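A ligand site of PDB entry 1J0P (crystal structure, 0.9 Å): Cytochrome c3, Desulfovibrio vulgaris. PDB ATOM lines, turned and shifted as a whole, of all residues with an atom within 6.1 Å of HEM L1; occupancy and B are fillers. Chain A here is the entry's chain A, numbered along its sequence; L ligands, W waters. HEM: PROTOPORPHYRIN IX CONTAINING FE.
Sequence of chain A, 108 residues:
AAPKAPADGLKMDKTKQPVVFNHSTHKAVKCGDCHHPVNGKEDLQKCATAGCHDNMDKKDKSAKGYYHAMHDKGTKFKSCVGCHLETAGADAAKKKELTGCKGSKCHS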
ATOM      1  N   MET A  12      34.230  13.154  34.818  1.00  0.00           N
ATOM      2  CA  MET A  12      34.353  14.556  35.217  1.00  0.00           C
ATOM      3  C   MET A  12      33.154  14.883  36.039  1.00  0.00           C
ATOM      4  O   MET A  12      32.032  14.840  35.496  1.00  0.00           O
ATOM      5  CB  MET A  12      34.518  15.424  33.992  1.00  0.00           C
ATOM      6  CG  MET A  12      35.687  15.049  33.126  1.00  0.00           C
ATOM      7  SD  MET A  12      35.852  16.036  31.637  1.00  0.00           S
ATOM      8  CE  MET A  12      36.507  17.549  32.318  1.00  0.00           C
ATOM      9  N   ASP A  13      33.313  15.115  37.338  1.00  0.00           N
ATOM     10  CA  ASP A  13      32.195  15.139  38.273  1.00  0.00           C
ATOM     11  C   ASP A  13      32.293  16.270  39.266  1.00  0.00           C
ATOM     12  O   ASP A  13      31.897  16.155  40.434  1.00  0.00           O
ATOM     13  CB  ASP A  13      32.012  13.807  38.993  1.00  0.00           C
ATOM     14  CG  ASP A  13      33.135  13.351  39.836  1.00  0.00           C
ATOM     15  OD1 ASP A  13      34.115  14.097  39.887  1.00  0.00           O
ATOM     16  OD2 ASP A  13      32.850  12.247  40.376  1.00  0.00           O
ATOM     17  N   LYS A  14      32.820  17.405  38.830  1.00  0.00           N
ATOM     18  CA  LYS A  14      32.820  18.598  39.642  1.00  0.00           C
ATOM     19  C   LYS A  14      31.412  19.209  39.802  1.00  0.00           C
ATOM     20  O   LYS A  14      31.197  19.991  40.725  1.00  0.00           O
ATOM     21  CB  LYS A  14      33.726  19.654  39.072  1.00  0.00           C
ATOM     22  CG  LYS A  14      35.111  19.212  38.858  1.00  0.00           C
ATOM     23  CD  LYS A  14      35.850  18.673  40.009  1.00  0.00           C
ATOM     24  CE  LYS A  14      36.005  19.681  41.064  1.00  0.00           C
ATOM     25  NZ  LYS A  14      37.003  19.224  42.076  1.00  0.00           N
ATOM     26  N   THR A  15      30.509  18.829  38.933  1.00  0.00           N
ATOM     27  CA  THR A  15      29.167  19.399  38.868  1.00  0.00           C
ATOM     28  C   THR A  15      28.120  18.303  38.996  1.00  0.00           C
ATOM     29  O   THR A  15      28.432  17.109  38.953  1.00  0.00           O
ATOM     30  CB  THR A  15      28.934  20.159  37.554  1.00  0.00           C
ATOM     31  OG1 THR A  15      28.655  19.270  36.499  1.00  0.00           O
ATOM     32  CG2 THR A  15      30.164  20.993  37.156  1.00  0.00           C
ATOM     33  N   LYS A  16      26.879  18.738  39.067  1.00  0.00           N
ATOM     34  CA  LYS A  16      25.760  17.818  39.087  1.00  0.00           C
ATOM     35  C   LYS A  16      25.351  17.329  37.690  1.00  0.00           C
ATOM     36  O   LYS A  16      24.405  16.563  37.573  1.00  0.00           O
ATOM     37  CB  LYS A  16      24.559  18.439  39.743  1.00  0.00           C
ATOM     38  CG  LYS A  16      24.927  18.779  41.233  1.00  0.00           C
ATOM     39  CD  LYS A  16      23.867  18.545  42.228  1.00  0.00           C
ATOM     40  CE  LYS A  16      22.805  19.582  41.994  1.00  0.00           C
ATOM     41  NZ  LYS A  16      21.620  19.761  42.824  1.00  0.00           N
ATOM     42  N   GLN A  17      26.020  17.631  36.646  1.00  0.00           N
ATOM     43  CA  GLN A  17      25.960  17.161  35.299  1.00  0.00           C
ATOM     44  C   GLN A  17      27.280  16.518  34.862  1.00  0.00           C
ATOM     45  O   GLN A  17      27.960  17.006  33.954  1.00  0.00           O
ATOM     46  CB  GLN A  17      25.567  18.281  34.313  1.00  0.00           C
ATOM     47  CG  GLN A  17      24.273  18.965  34.685  1.00  0.00           C
ATOM     48  CD  GLN A  17      23.041  18.097  34.442  1.00  0.00           C
ATOM     49  OE1 GLN A  17      23.101  16.954  33.834  1.00  0.00           O
ATOM     50  NE2 GLN A  17      21.997  18.583  34.873  1.00  0.00           N
ATOM     51  N   PRO A  18      27.668  15.390  35.513  1.00  0.00           N
ATOM     52  CA  PRO A  18      28.923  14.773  35.181  1.00  0.00           C
ATOM     53  C   PRO A  18      29.010  14.281  33.759  1.00  0.00           C
ATOM     54  O   PRO A  18      27.990  13.974  33.142  1.00  0.00           O
ATOM     55  CB  PRO A  18      29.047  13.648  36.201  1.00  0.00           C
ATOM     56  CG  PRO A  18      27.631  13.360  36.608  1.00  0.00           C
ATOM     57  CD  PRO A  18      26.960  14.675  36.581  1.00  0.00           C
ATOM     58  N   VAL A  19      30.245  14.185  33.272  1.00  0.00           N
ATOM     59  CA  VAL A  19      30.531  13.798  31.874  1.00  0.00           C
ATOM     60  C   VAL A  19      31.666  12.807  31.859  1.00  0.00           C
ATOM     61  O   VAL A  19      32.685  13.040  32.532  1.00  0.00           O
ATOM     62  CB  VAL A  19      30.870  15.044  31.078  1.00  0.00           C
ATOM     63  CG1 VAL A  19      31.321  14.706  29.643  1.00  0.00           C
ATOM     64  CG2 VAL A  19      29.694  15.986  31.013  1.00  0.00           C
ATOM     65  N   MET A  56      33.302  27.399  40.142  1.00  0.00           N
ATOM     66  CA  MET A  56      32.125  26.640  39.840  1.00  0.00           C
ATOM     67  C   MET A  56      30.904  27.501  39.556  1.00  0.00           C
ATOM     68  O   MET A  56      29.827  26.970  39.379  1.00  0.00           O
ATOM     69  CB  MET A  56      31.851  25.629  40.983  1.00  0.00           C
ATOM     70  CG  MET A  56      32.988  24.586  41.108  1.00  0.00           C
ATOM     71  SD  MET A  56      33.093  23.548  39.626  1.00  0.00           S
ATOM     72  CE  MET A  56      34.796  23.421  39.350  1.00  0.00           C
ATOM     73  N   ASP A  57      31.106  28.809  39.403  1.00  0.00           N
ATOM     74  CA  ASP A  57      30.129  29.718  38.857  1.00  0.00           C
ATOM     75  C   ASP A  57      30.090  29.548  37.352  1.00  0.00           C
ATOM     76  O   ASP A  57      31.000  30.009  36.624  1.00  0.00           O
ATOM     77  CB  ASP A  57      30.503  31.150  39.171  1.00  0.00           C
ATOM     78  CG  ASP A  57      29.610  32.189  38.553  1.00  0.00           C
ATOM     79  OD1 ASP A  57      28.532  31.788  38.020  1.00  0.00           O
ATOM     80  OD2 ASP A  57      29.973  33.366  38.576  1.00  0.00           O
ATOM     81  N   LYS A  58      29.018  28.918  36.824  1.00  0.00           N
ATOM     82  CA  LYS A  58      28.916  28.637  35.437  1.00  0.00           C
ATOM     83  C   LYS A  58      28.743  29.909  34.577  1.00  0.00           C
ATOM     84  O   LYS A  58      28.808  29.839  33.356  1.00  0.00           O
ATOM     85  CB  LYS A  58      27.787  27.658  35.124  1.00  0.00           C
ATOM     86  CG  LYS A  58      26.378  28.257  35.151  1.00  0.00           C
ATOM     87  CD  LYS A  58      25.297  27.224  34.728  1.00  0.00           C
ATOM     88  CE  LYS A  58      23.964  27.947  34.661  1.00  0.00           C
ATOM     89  NZ  LYS A  58      22.909  26.982  34.150  1.00  0.00           N
ATOM     90  N   TYR A  66      35.131  27.103  35.213  1.00  0.00           N
ATOM     91  CA  TYR A  66      35.142  25.711  34.785  1.00  0.00           C
ATOM     92  C   TYR A  66      34.159  25.454  33.637  1.00  0.00           C
ATOM     93  O   TYR A  66      34.521  24.869  32.625  1.00  0.00           O
ATOM     94  CB  TYR A  66      34.862  24.839  36.003  1.00  0.00           C
ATOM     95  CG  TYR A  66      34.893  23.346  35.739  1.00  0.00           C
ATOM     96  CD1 TYR A  66      33.728  22.596  35.766  1.00  0.00           C
ATOM     97  CD2 TYR A  66      36.091  22.664  35.550  1.00  0.00           C
ATOM     98  CE1 TYR A  66      33.759  21.243  35.571  1.00  0.00           C
ATOM     99  CE2 TYR A  66      36.091  21.311  35.328  1.00  0.00           C
ATOM    100  CZ  TYR A  66      34.918  20.588  35.325  1.00  0.00           C
ATOM    101  OH  TYR A  66      34.983  19.234  35.119  1.00  0.00           O
ATOM    102  N   TYR A  67      32.899  25.902  33.800  1.00  0.00           N
ATOM    103  CA  TYR A  67      31.953  25.741  32.708  1.00  0.00           C
ATOM    104  C   TYR A  67      32.492  26.385  31.447  1.00  0.00           C
ATOM    105  O   TYR A  67      32.433  25.808  30.352  1.00  0.00           O
ATOM    106  CB  TYR A  67      30.598  26.402  33.131  1.00  0.00           C
ATOM    107  CG  TYR A  67      29.551  26.305  32.039  1.00  0.00           C
ATOM    108  CD1 TYR A  67      29.514  27.203  30.975  1.00  0.00           C
ATOM    109  CD2 TYR A  67      28.598  25.323  32.062  1.00  0.00           C
ATOM    110  CE1 TYR A  67      28.582  27.104  29.969  1.00  0.00           C
ATOM    111  CE2 TYR A  67      27.643  25.209  31.047  1.00  0.00           C
ATOM    112  CZ  TYR A  67      27.647  26.112  30.031  1.00  0.00           C
ATOM    113  OH  TYR A  67      26.676  25.951  29.051  1.00  0.00           O
ATOM    114  N   MET A  70      35.021  24.414  29.486  1.00  0.00           N
ATOM    115  CA  MET A  70      34.506  23.209  28.828  1.00  0.00           C
ATOM    116  C   MET A  70      33.547  23.535  27.688  1.00  0.00           C
ATOM    117  O   MET A  70      33.378  22.655  26.809  1.00  0.00           O
ATOM    118  CB  MET A  70      33.778  22.294  29.830  1.00  0.00           C
ATOM    119  CG  MET A  70      34.651  21.919  31.009  1.00  0.00           C
ATOM    120  SD  MET A  70      36.188  21.084  30.576  1.00  0.00           S
ATOM    121  CE  MET A  70      37.215  21.533  31.903  1.00  0.00           C
ATOM    122  N   HIS A  71      32.917  24.718  27.629  1.00  0.00           N
ATOM    123  CA  HIS A  71      31.800  24.962  26.715  1.00  0.00           C
ATOM    124  C   HIS A  71      32.023  26.068  25.686  1.00  0.00           C
ATOM    125  O   HIS A  71      31.257  26.085  24.715  1.00  0.00           O
ATOM    126  CB  HIS A  71      30.506  25.251  27.477  1.00  0.00           C
ATOM    127  CG  HIS A  71      30.031  24.153  28.331  1.00  0.00           C
ATOM    128  ND1 HIS A  71      30.508  23.937  29.613  1.00  0.00           N
ATOM    129  CD2 HIS A  71      29.120  23.175  28.126  1.00  0.00           C
ATOM    130  CE1 HIS A  71      29.892  22.851  30.110  1.00  0.00           C
ATOM    131  NE2 HIS A  71      29.024  22.349  29.218  1.00  0.00           N
ATOM    132  N   CYS A  80      35.958  21.633  25.053  1.00  0.00           N
ATOM    133  CA  CYS A  80      35.260  20.441  24.623  1.00  0.00           C
ATOM    134  C   CYS A  80      34.242  20.801  23.503  1.00  0.00           C
ATOM    135  O   CYS A  80      34.220  20.200  22.451  1.00  0.00           O
ATOM    136  CB  CYS A  80      34.491  19.772  25.751  1.00  0.00           C
ATOM    137  SG  CYS A  80      35.316  19.519  27.339  1.00  0.00           S
ATOM    138  N   VAL A  81      33.333  21.736  23.838  1.00  0.00           N
ATOM    139  CA  VAL A  81      32.274  22.070  22.904  1.00  0.00           C
ATOM    140  C   VAL A  81      32.827  22.757  21.673  1.00  0.00           C
ATOM    141  O   VAL A  81      32.397  22.487  20.560  1.00  0.00           O
ATOM    142  CB  VAL A  81      31.154  22.870  23.544  1.00  0.00           C
ATOM    143  CG1 VAL A  81      30.097  23.256  22.513  1.00  0.00           C
ATOM    144  CG2 VAL A  81      30.497  22.091  24.689  1.00  0.00           C
ATOM    145  N   HIS A  84      34.313  20.251  19.393  1.00  0.00           N
ATOM    146  CA  HIS A  84      33.251  19.400  18.836  1.00  0.00           C
ATOM    147  C   HIS A  84      32.379  20.137  17.791  1.00  0.00           C
ATOM    148  O   HIS A  84      31.935  19.517  16.825  1.00  0.00           O
ATOM    149  CB  HIS A  84      32.376  18.889  19.957  1.00  0.00           C
ATOM    150  CG  HIS A  84      33.013  17.763  20.742  1.00  0.00           C
ATOM    151  ND1 HIS A  84      32.221  16.953  21.490  1.00  0.00           N
ATOM    152  CD2 HIS A  84      34.284  17.314  20.905  1.00  0.00           C
ATOM    153  CE1 HIS A  84      33.009  16.083  22.103  1.00  0.00           C
ATOM    154  NE2 HIS A  84      34.292  16.245  21.780  1.00  0.00           N
ATOM    155  N   GLU A  97      25.027  14.539  18.586  1.00  0.00           N
ATOM    156  CA  GLU A  97      25.847  13.621  19.354  1.00  0.00           C
ATOM    157  C   GLU A  97      26.983  14.283  20.124  1.00  0.00           C
ATOM    158  O   GLU A  97      27.297  13.946  21.252  1.00  0.00           O
ATOM    159  CB  GLU A  97      26.430  12.609  18.335  1.00  0.00           C
ATOM    160  CG  GLU A  97      27.251  11.466  18.906  1.00  0.00           C
ATOM    161  CD  GLU A  97      28.078  10.666  17.910  1.00  0.00           C
ATOM    162  OE1 GLU A  97      28.984   9.861  18.209  1.00  0.00           O
ATOM    163  OE2 GLU A  97      27.787  10.844  16.744  1.00  0.00           O
ATOM    164  N   LEU A  98      27.629  15.256  19.467  1.00  0.00           N
ATOM    165  CA  LEU A  98      28.854  15.835  20.001  1.00  0.00           C
ATOM    166  C   LEU A  98      28.689  17.190  20.636  1.00  0.00           C
ATOM    167  O   LEU A  98      29.577  17.568  21.426  1.00  0.00           O
ATOM    168  CB  LEU A  98      29.880  15.963  18.846  1.00  0.00           C
ATOM    169  CG  LEU A  98      30.276  14.685  18.152  1.00  0.00           C
ATOM    170  CD1 LEU A  98      31.240  14.962  17.014  1.00  0.00           C
ATOM    171  CD2 LEU A  98      30.876  13.658  19.115  1.00  0.00           C
ATOM    172  N   THR A  99      27.599  17.920  20.356  1.00  0.00           N
ATOM    173  CA  THR A  99      27.424  19.278  20.891  1.00  0.00           C
ATOM    174  C   THR A  99      26.099  19.472  21.590  1.00  0.00           C
ATOM    175  O   THR A  99      25.907  20.544  22.169  1.00  0.00           O
ATOM    176  CB  THR A  99      27.656  20.357  19.840  1.00  0.00           C
ATOM    177  OG1 THR A  99      26.562  20.463  18.930  1.00  0.00           O
ATOM    178  CG2 THR A  99      28.929  20.131  19.080  1.00  0.00           C
ATOM    179  N   GLY A 100      25.187  18.502  21.583  1.00  0.00           N
ATOM    180  CA  GLY A 100      23.886  18.731  22.201  1.00  0.00           C
ATOM    181  C   GLY A 100      23.999  18.946  23.696  1.00  0.00           C
ATOM    182  O   GLY A 100      24.782  18.308  24.385  1.00  0.00           O
ATOM    183  N   CYS A 101      23.127  19.798  24.198  1.00  0.00           N
ATOM    184  CA  CYS A 101      23.129  20.101  25.634  1.00  0.00           C
ATOM    185  C   CYS A 101      22.529  18.980  26.471  1.00  0.00           C
ATOM    186  O   CYS A 101      22.799  18.911  27.671  1.00  0.00           O
ATOM    187  CB  CYS A 101      22.426  21.397  25.948  1.00  0.00           C
ATOM    188  SG  CYS A 101      23.019  22.830  25.009  1.00  0.00           S
ATOM    189  N   LYS A 102      21.692  18.158  25.845  1.00  0.00           N
ATOM    190  CA  LYS A 102      21.099  17.001  26.513  1.00  0.00           C
ATOM    191  C   LYS A 102      21.013  15.917  25.443  1.00  0.00           C
ATOM    192  O   LYS A 102      21.042  16.186  24.244  1.00  0.00           O
ATOM    193  CB  LYS A 102      19.749  17.250  27.117  1.00  0.00           C
ATOM    194  CG  LYS A 102      18.673  17.560  26.114  1.00  0.00           C
ATOM    195  CD  LYS A 102      17.322  17.799  26.716  1.00  0.00           C
ATOM    196  CE  LYS A 102      16.158  17.636  25.662  1.00  0.00           C
ATOM    197  NZ  LYS A 102      15.886  16.233  25.347  1.00  0.00           N
ATOM    198  N   SER A 104      23.198  13.883  24.475  1.00  0.00           N
ATOM    199  CA  SER A 104      24.431  13.853  23.690  1.00  0.00           C
ATOM    200  C   SER A 104      25.383  12.886  24.327  1.00  0.00           C
ATOM    201  O   SER A 104      25.144  12.348  25.408  1.00  0.00           O
ATOM    202  CB  SER A 104      25.012  15.251  23.529  1.00  0.00           C
ATOM    203  OG  SER A 104      25.504  15.710  24.782  1.00  0.00           O
ATOM    204  N   LYS A 105      26.511  12.689  23.658  1.00  0.00           N
ATOM    205  CA  LYS A 105      27.520  11.825  24.263  1.00  0.00           C
ATOM    206  C   LYS A 105      28.161  12.446  25.491  1.00  0.00           C
ATOM    207  O   LYS A 105      28.763  11.742  26.294  1.00  0.00           O
ATOM    208  CB  LYS A 105      28.542  11.333  23.257  1.00  0.00           C
ATOM    209  CG  LYS A 105      27.845  10.410  22.212  1.00  0.00           C
ATOM    210  CD  LYS A 105      28.845   9.704  21.348  1.00  0.00           C
ATOM    211  CE  LYS A 105      28.237   8.548  20.563  1.00  0.00           C
ATOM    212  NZ  LYS A 105      28.037   7.313  21.372  1.00  0.00           N
ATOM    213  N   CYS A 106      28.114  13.801  25.593  1.00  0.00           N
ATOM    214  CA  CYS A 106      28.572  14.431  26.837  1.00  0.00           C
ATOM    215  C   CYS A 106      27.529  14.339  27.929  1.00  0.00           C
ATOM    216  O   CYS A 106      27.830  13.882  29.045  1.00  0.00           O
ATOM    217  CB  CYS A 106      28.922  15.885  26.590  1.00  0.00           C
ATOM    218  SG  CYS A 106      30.338  16.021  25.465  1.00  0.00           S
ATOM    219  N   HIS A 107      26.343  14.843  27.699  1.00  0.00           N
ATOM    220  CA  HIS A 107      25.234  14.872  28.656  1.00  0.00           C
ATOM    221  C   HIS A 107      24.217  13.869  28.199  1.00  0.00           C
ATOM    222  O   HIS A 107      23.336  14.215  27.392  1.00  0.00           O
ATOM    223  CB  HIS A 107      24.644  16.253  28.798  1.00  0.00           C
ATOM    224  CG  HIS A 107      25.620  17.275  29.329  1.00  0.00           C
ATOM    225  ND1 HIS A 107      26.199  17.178  30.579  1.00  0.00           N
ATOM    226  CD2 HIS A 107      26.082  18.431  28.787  1.00  0.00           C
ATOM    227  CE1 HIS A 107      26.987  18.239  30.754  1.00  0.00           C
ATOM    228  NE2 HIS A 107      26.940  19.047  29.684  1.00  0.00           N
HETATM  229  CHA HEM L   1      28.838  20.529  32.773  1.00  0.00           C
HETATM  230  CHB HEM L   1      25.299  22.641  30.239  1.00  0.00           C
HETATM  231  CHC HEM L   1      26.956  20.736  26.207  1.00  0.00           C
HETATM  232  CHD HEM L   1      30.747  19.017  28.643  1.00  0.00           C
HETATM  233  C1A HEM L   1      27.651  21.187  32.454  1.00  0.00           C
HETATM  234  C2A HEM L   1      26.735  21.792  33.404  1.00  0.00           C
HETATM  235  C3A HEM L   1      25.757  22.354  32.699  1.00  0.00           C
HETATM  236  C4A HEM L   1      26.023  22.127  31.288  1.00  0.00           C
HETATM  237  CMA HEM L   1      24.539  23.147  33.148  1.00  0.00           C
HETATM  238  CAA HEM L   1      26.906  21.794  34.898  1.00  0.00           C
HETATM  239  CBA HEM L   1      27.378  23.176  35.381  1.00  0.00           C
HETATM  240  CGA HEM L   1      27.335  23.327  36.881  1.00  0.00           C
HETATM  241  O1A HEM L   1      26.289  22.983  37.479  1.00  0.00           O
HETATM  242  O2A HEM L   1      28.365  23.737  37.493  1.00  0.00           O
HETATM  243  C1B HEM L   1      25.554  22.433  28.928  1.00  0.00           C
HETATM  244  C2B HEM L   1      24.797  23.033  27.887  1.00  0.00           C
HETATM  245  C3B HEM L   1      25.231  22.487  26.703  1.00  0.00           C
HETATM  246  C4B HEM L   1      26.272  21.539  27.061  1.00  0.00           C
HETATM  247  CMB HEM L   1      23.764  24.147  28.083  1.00  0.00           C
HETATM  248  CAB HEM L   1      24.844  22.775  25.322  1.00  0.00           C
HETATM  249  CBB HEM L   1      25.356  24.081  24.774  1.00  0.00           C
HETATM  250  C1C HEM L   1      28.040  19.950  26.555  1.00  0.00           C
HETATM  251  C2C HEM L   1      28.744  19.105  25.646  1.00  0.00           C
HETATM  252  C3C HEM L   1      29.882  18.626  26.300  1.00  0.00           C
HETATM  253  C4C HEM L   1      29.801  19.197  27.644  1.00  0.00           C
HETATM  254  CMC HEM L   1      28.258  18.791  24.243  1.00  0.00           C
HETATM  255  CAC HEM L   1      30.904  17.717  25.788  1.00  0.00           C
HETATM  256  CBC HEM L   1      31.572  18.208  24.540  1.00  0.00           C
HETATM  257  C1D HEM L   1      30.602  19.394  29.963  1.00  0.00           C
HETATM  258  C2D HEM L   1      31.589  19.111  30.986  1.00  0.00           C
HETATM  259  C3D HEM L   1      31.028  19.469  32.159  1.00  0.00           C
HETATM  260  C4D HEM L   1      29.717  20.016  31.853  1.00  0.00           C
HETATM  261  CMD HEM L   1      32.905  18.448  30.741  1.00  0.00           C
HETATM  262  CAD HEM L   1      31.564  19.317  33.538  1.00  0.00           C
HETATM  263  CBD HEM L   1      31.283  17.923  34.128  1.00  0.00           C
HETATM  264  CGD HEM L   1      31.669  17.835  35.584  1.00  0.00           C
HETATM  265  O1D HEM L   1      32.834  18.031  35.969  1.00  0.00           O
HETATM  266  O2D HEM L   1      30.715  17.616  36.407  1.00  0.00           O
HETATM  267  NA  HEM L   1      27.184  21.407  31.195  1.00  0.00           N
HETATM  268  NB  HEM L   1      26.451  21.550  28.417  1.00  0.00           N
HETATM  269  NC  HEM L   1      28.683  19.969  27.754  1.00  0.00           N
HETATM  270  ND  HEM L   1      29.506  19.953  30.517  1.00  0.00           N
HETATM  271 FE   HEM L   1      27.956  20.714  29.464  1.00  0.00          FE
HETATM  272  CHA HEM L   2      34.448  12.536  20.694  1.00  0.00           C
HETATM  273  CHB HEM L   2      33.893  14.380  25.094  1.00  0.00           C
HETATM  274  CHC HEM L   2      37.297  17.601  24.123  1.00  0.00           C
HETATM  275  CHD HEM L   2      37.507  16.087  19.585  1.00  0.00           C
HETATM  276  C1A HEM L   2      33.983  12.742  21.985  1.00  0.00           C
HETATM  277  C2A HEM L   2      32.951  11.995  22.627  1.00  0.00           C
HETATM  278  C3A HEM L   2      32.774  12.513  23.843  1.00  0.00           C
HETATM  279  C4A HEM L   2      33.725  13.579  24.000  1.00  0.00           C
HETATM  280  CMA HEM L   2      31.809  12.122  24.941  1.00  0.00           C
HETATM  281  CAA HEM L   2      32.240  10.838  21.952  1.00  0.00           C
HETATM  282  CBA HEM L   2      33.089   9.569  22.003  1.00  0.00           C
HETATM  283  CGA HEM L   2      33.239   9.024  23.417  1.00  0.00           C
HETATM  284  O1A HEM L   2      32.224   8.490  23.874  1.00  0.00           O
HETATM  285  O2A HEM L   2      34.307   9.174  24.017  1.00  0.00           O
HETATM  286  C1B HEM L   2      34.772  15.412  25.212  1.00  0.00           C
HETATM  287  C2B HEM L   2      34.927  16.218  26.388  1.00  0.00           C
HETATM  288  C3B HEM L   2      35.942  17.117  26.145  1.00  0.00           C
HETATM  289  C4B HEM L   2      36.367  16.857  24.788  1.00  0.00           C
HETATM  290  CMB HEM L   2      34.097  16.082  27.657  1.00  0.00           C
HETATM  291  CAB HEM L   2      36.512  18.168  27.004  1.00  0.00           C
HETATM  292  CBB HEM L   2      37.028  17.705  28.357  1.00  0.00           C
HETATM  293  C1C HEM L   2      37.642  17.520  22.798  1.00  0.00           C
HETATM  294  C2C HEM L   2      38.551  18.424  22.120  1.00  0.00           C
HETATM  295  C3C HEM L   2      38.583  18.000  20.791  1.00  0.00           C
HETATM  296  C4C HEM L   2      37.703  16.847  20.711  1.00  0.00           C
HETATM  297  CMC HEM L   2      39.199  19.589  22.795  1.00  0.00           C
HETATM  298  CAC HEM L   2      39.240  18.601  19.613  1.00  0.00           C
HETATM  299  CBC HEM L   2      40.469  19.415  19.872  1.00  0.00           C
HETATM  300  C1D HEM L   2      36.751  14.946  19.520  1.00  0.00           C
HETATM  301  C2D HEM L   2      36.628  14.119  18.329  1.00  0.00           C
HETATM  302  C3D HEM L   2      35.783  13.130  18.655  1.00  0.00           C
HETATM  303  C4D HEM L   2      35.332  13.341  20.011  1.00  0.00           C
HETATM  304  CMD HEM L   2      37.334  14.389  17.035  1.00  0.00           C
HETATM  305  CAD HEM L   2      35.263  12.014  17.778  1.00  0.00           C
HETATM  306  CBD HEM L   2      34.031  12.469  17.001  1.00  0.00           C
HETATM  307  CGD HEM L   2      33.189  11.365  16.391  1.00  0.00           C
HETATM  308  O1D HEM L   2      33.124  10.263  16.988  1.00  0.00           O
HETATM  309  O2D HEM L   2      32.417  11.643  15.459  1.00  0.00           O
HETATM  310  NA  HEM L   2      34.457  13.692  22.842  1.00  0.00           N
HETATM  311  NB  HEM L   2      35.627  15.849  24.250  1.00  0.00           N
HETATM  312  NC  HEM L   2      37.138  16.627  21.934  1.00  0.00           N
HETATM  313  ND  HEM L   2      35.946  14.429  20.489  1.00  0.00           N
HETATM  314 FE   HEM L   2      35.783  15.139  22.373  1.00  0.00          FE
HETATM  315  O   HOH W   1      27.048  25.661  22.176  1.00  0.00           O
HETATM  316  O   HOH W   2      26.273  21.459  39.641  1.00  0.00           O
HETATM  317  O   HOH W   3      23.728  22.581  36.696  1.00  0.00           O
HETATM  318  O   HOH W   4      29.121  24.216  39.872  1.00  0.00           O
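The backbone NH (N) of Asp 13 is in hydrogen-bond range of an oxygen (O1D) of HEM L1 (3.3 Å).
An oxygen (O2D) of HEM L1 sits at hydrogen-bond distance from the side-chain hydroxyl of Thr 15 (2.6 Å).
CAC of HEM L1 is bonded to SG of Cys 106, at 1.8 Å.
The side-chain hydroxyl (OH) of Tyr 66 is in hydrogen-bond range of an oxygen (O1D) of HEM L1.
NE2 of His 107 binds FE of HEM L1 (2.0 Å).
FE of HEM L1 is bound by NE2 of His 71 (2.0 Å).
N of Thr 15 sits at hydrogen-bond distance from O2D of HEM L1, at 2.8 Å.
The side-chain sulfur (SG) of Cys 80 is covalently linked to a carbon (CAB) of HEM L2 (1.8 Å).
The backbone NH (N) of Lys 14 is in hydrogen-bond range of an oxygen (O1D) of HEM L1 (2.9 Å).
A ring nitrogen (NE2) of His 84 binds an iron atom (FE) of HEM L2, 1.9 Å away.
A carbon (CAB) of HEM L1 is bonded to the side-chain sulfur of Cys 101.
O of Met 12 lies close to O2D of HEM L1 (3.2 Å).
Residues that only touch HEM L1: Leu 98, His 84, Gln 17, Thr 99, Tyr 67, Gly 100, Cys 80, Pro 18, Val 81, Val 19 and Met 70.
Within 4 Å of HEM L1: Met 12, Asp 13, Lys 14, Thr 15, Gln 17, Pro 18, Val 19, Tyr 66, Tyr 67, Met 70, His 71, Cys 80, Val 81, His 84, Leu 98, Thr 99, Gly 100, Cys 101, Cys 106 and His 107.
N of Cys 106 sits close to OG of Ser 104 (3.3 Å).
The backbone carbonyl oxygen of Gly 100 lies within hydrogen-bond range of the side-chain hydroxyl of Ser 104.
A ring nitrogen (ND1) of His 84 is in hydrogen-bond range of the backbone carbonyl oxygen (O) of Leu 98.
O of Met 70 sits close to N of Cys 80 (3.3 Å).
OG1 of Thr 15 sits at hydrogen-bond distance from N of Gln 17, 3.1 Å away.
OG of Ser 104 sits at hydrogen-bond distance from N of His 107, at 3.2 Å.
ND1 of His 71 sits at hydrogen-bond distance from O of Tyr 67, 2.8 Å away.
The backbone carbonyl oxygen of Val 19 is in hydrogen-bond range of the backbone NH of Met 12 (2.8 Å).
Water W4 lies within hydrogen-bond range of an oxygen (O2A) of HEM L1 (2.5 Å) and the backbone carbonyl oxygen (O) of Met 56 (2.9 Å).
Water W2 lies within hydrogen-bond range of an oxygen (O1A) of HEM L1 (2.6 Å) and the backbone NH of Lys 16 (2.8 Å).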
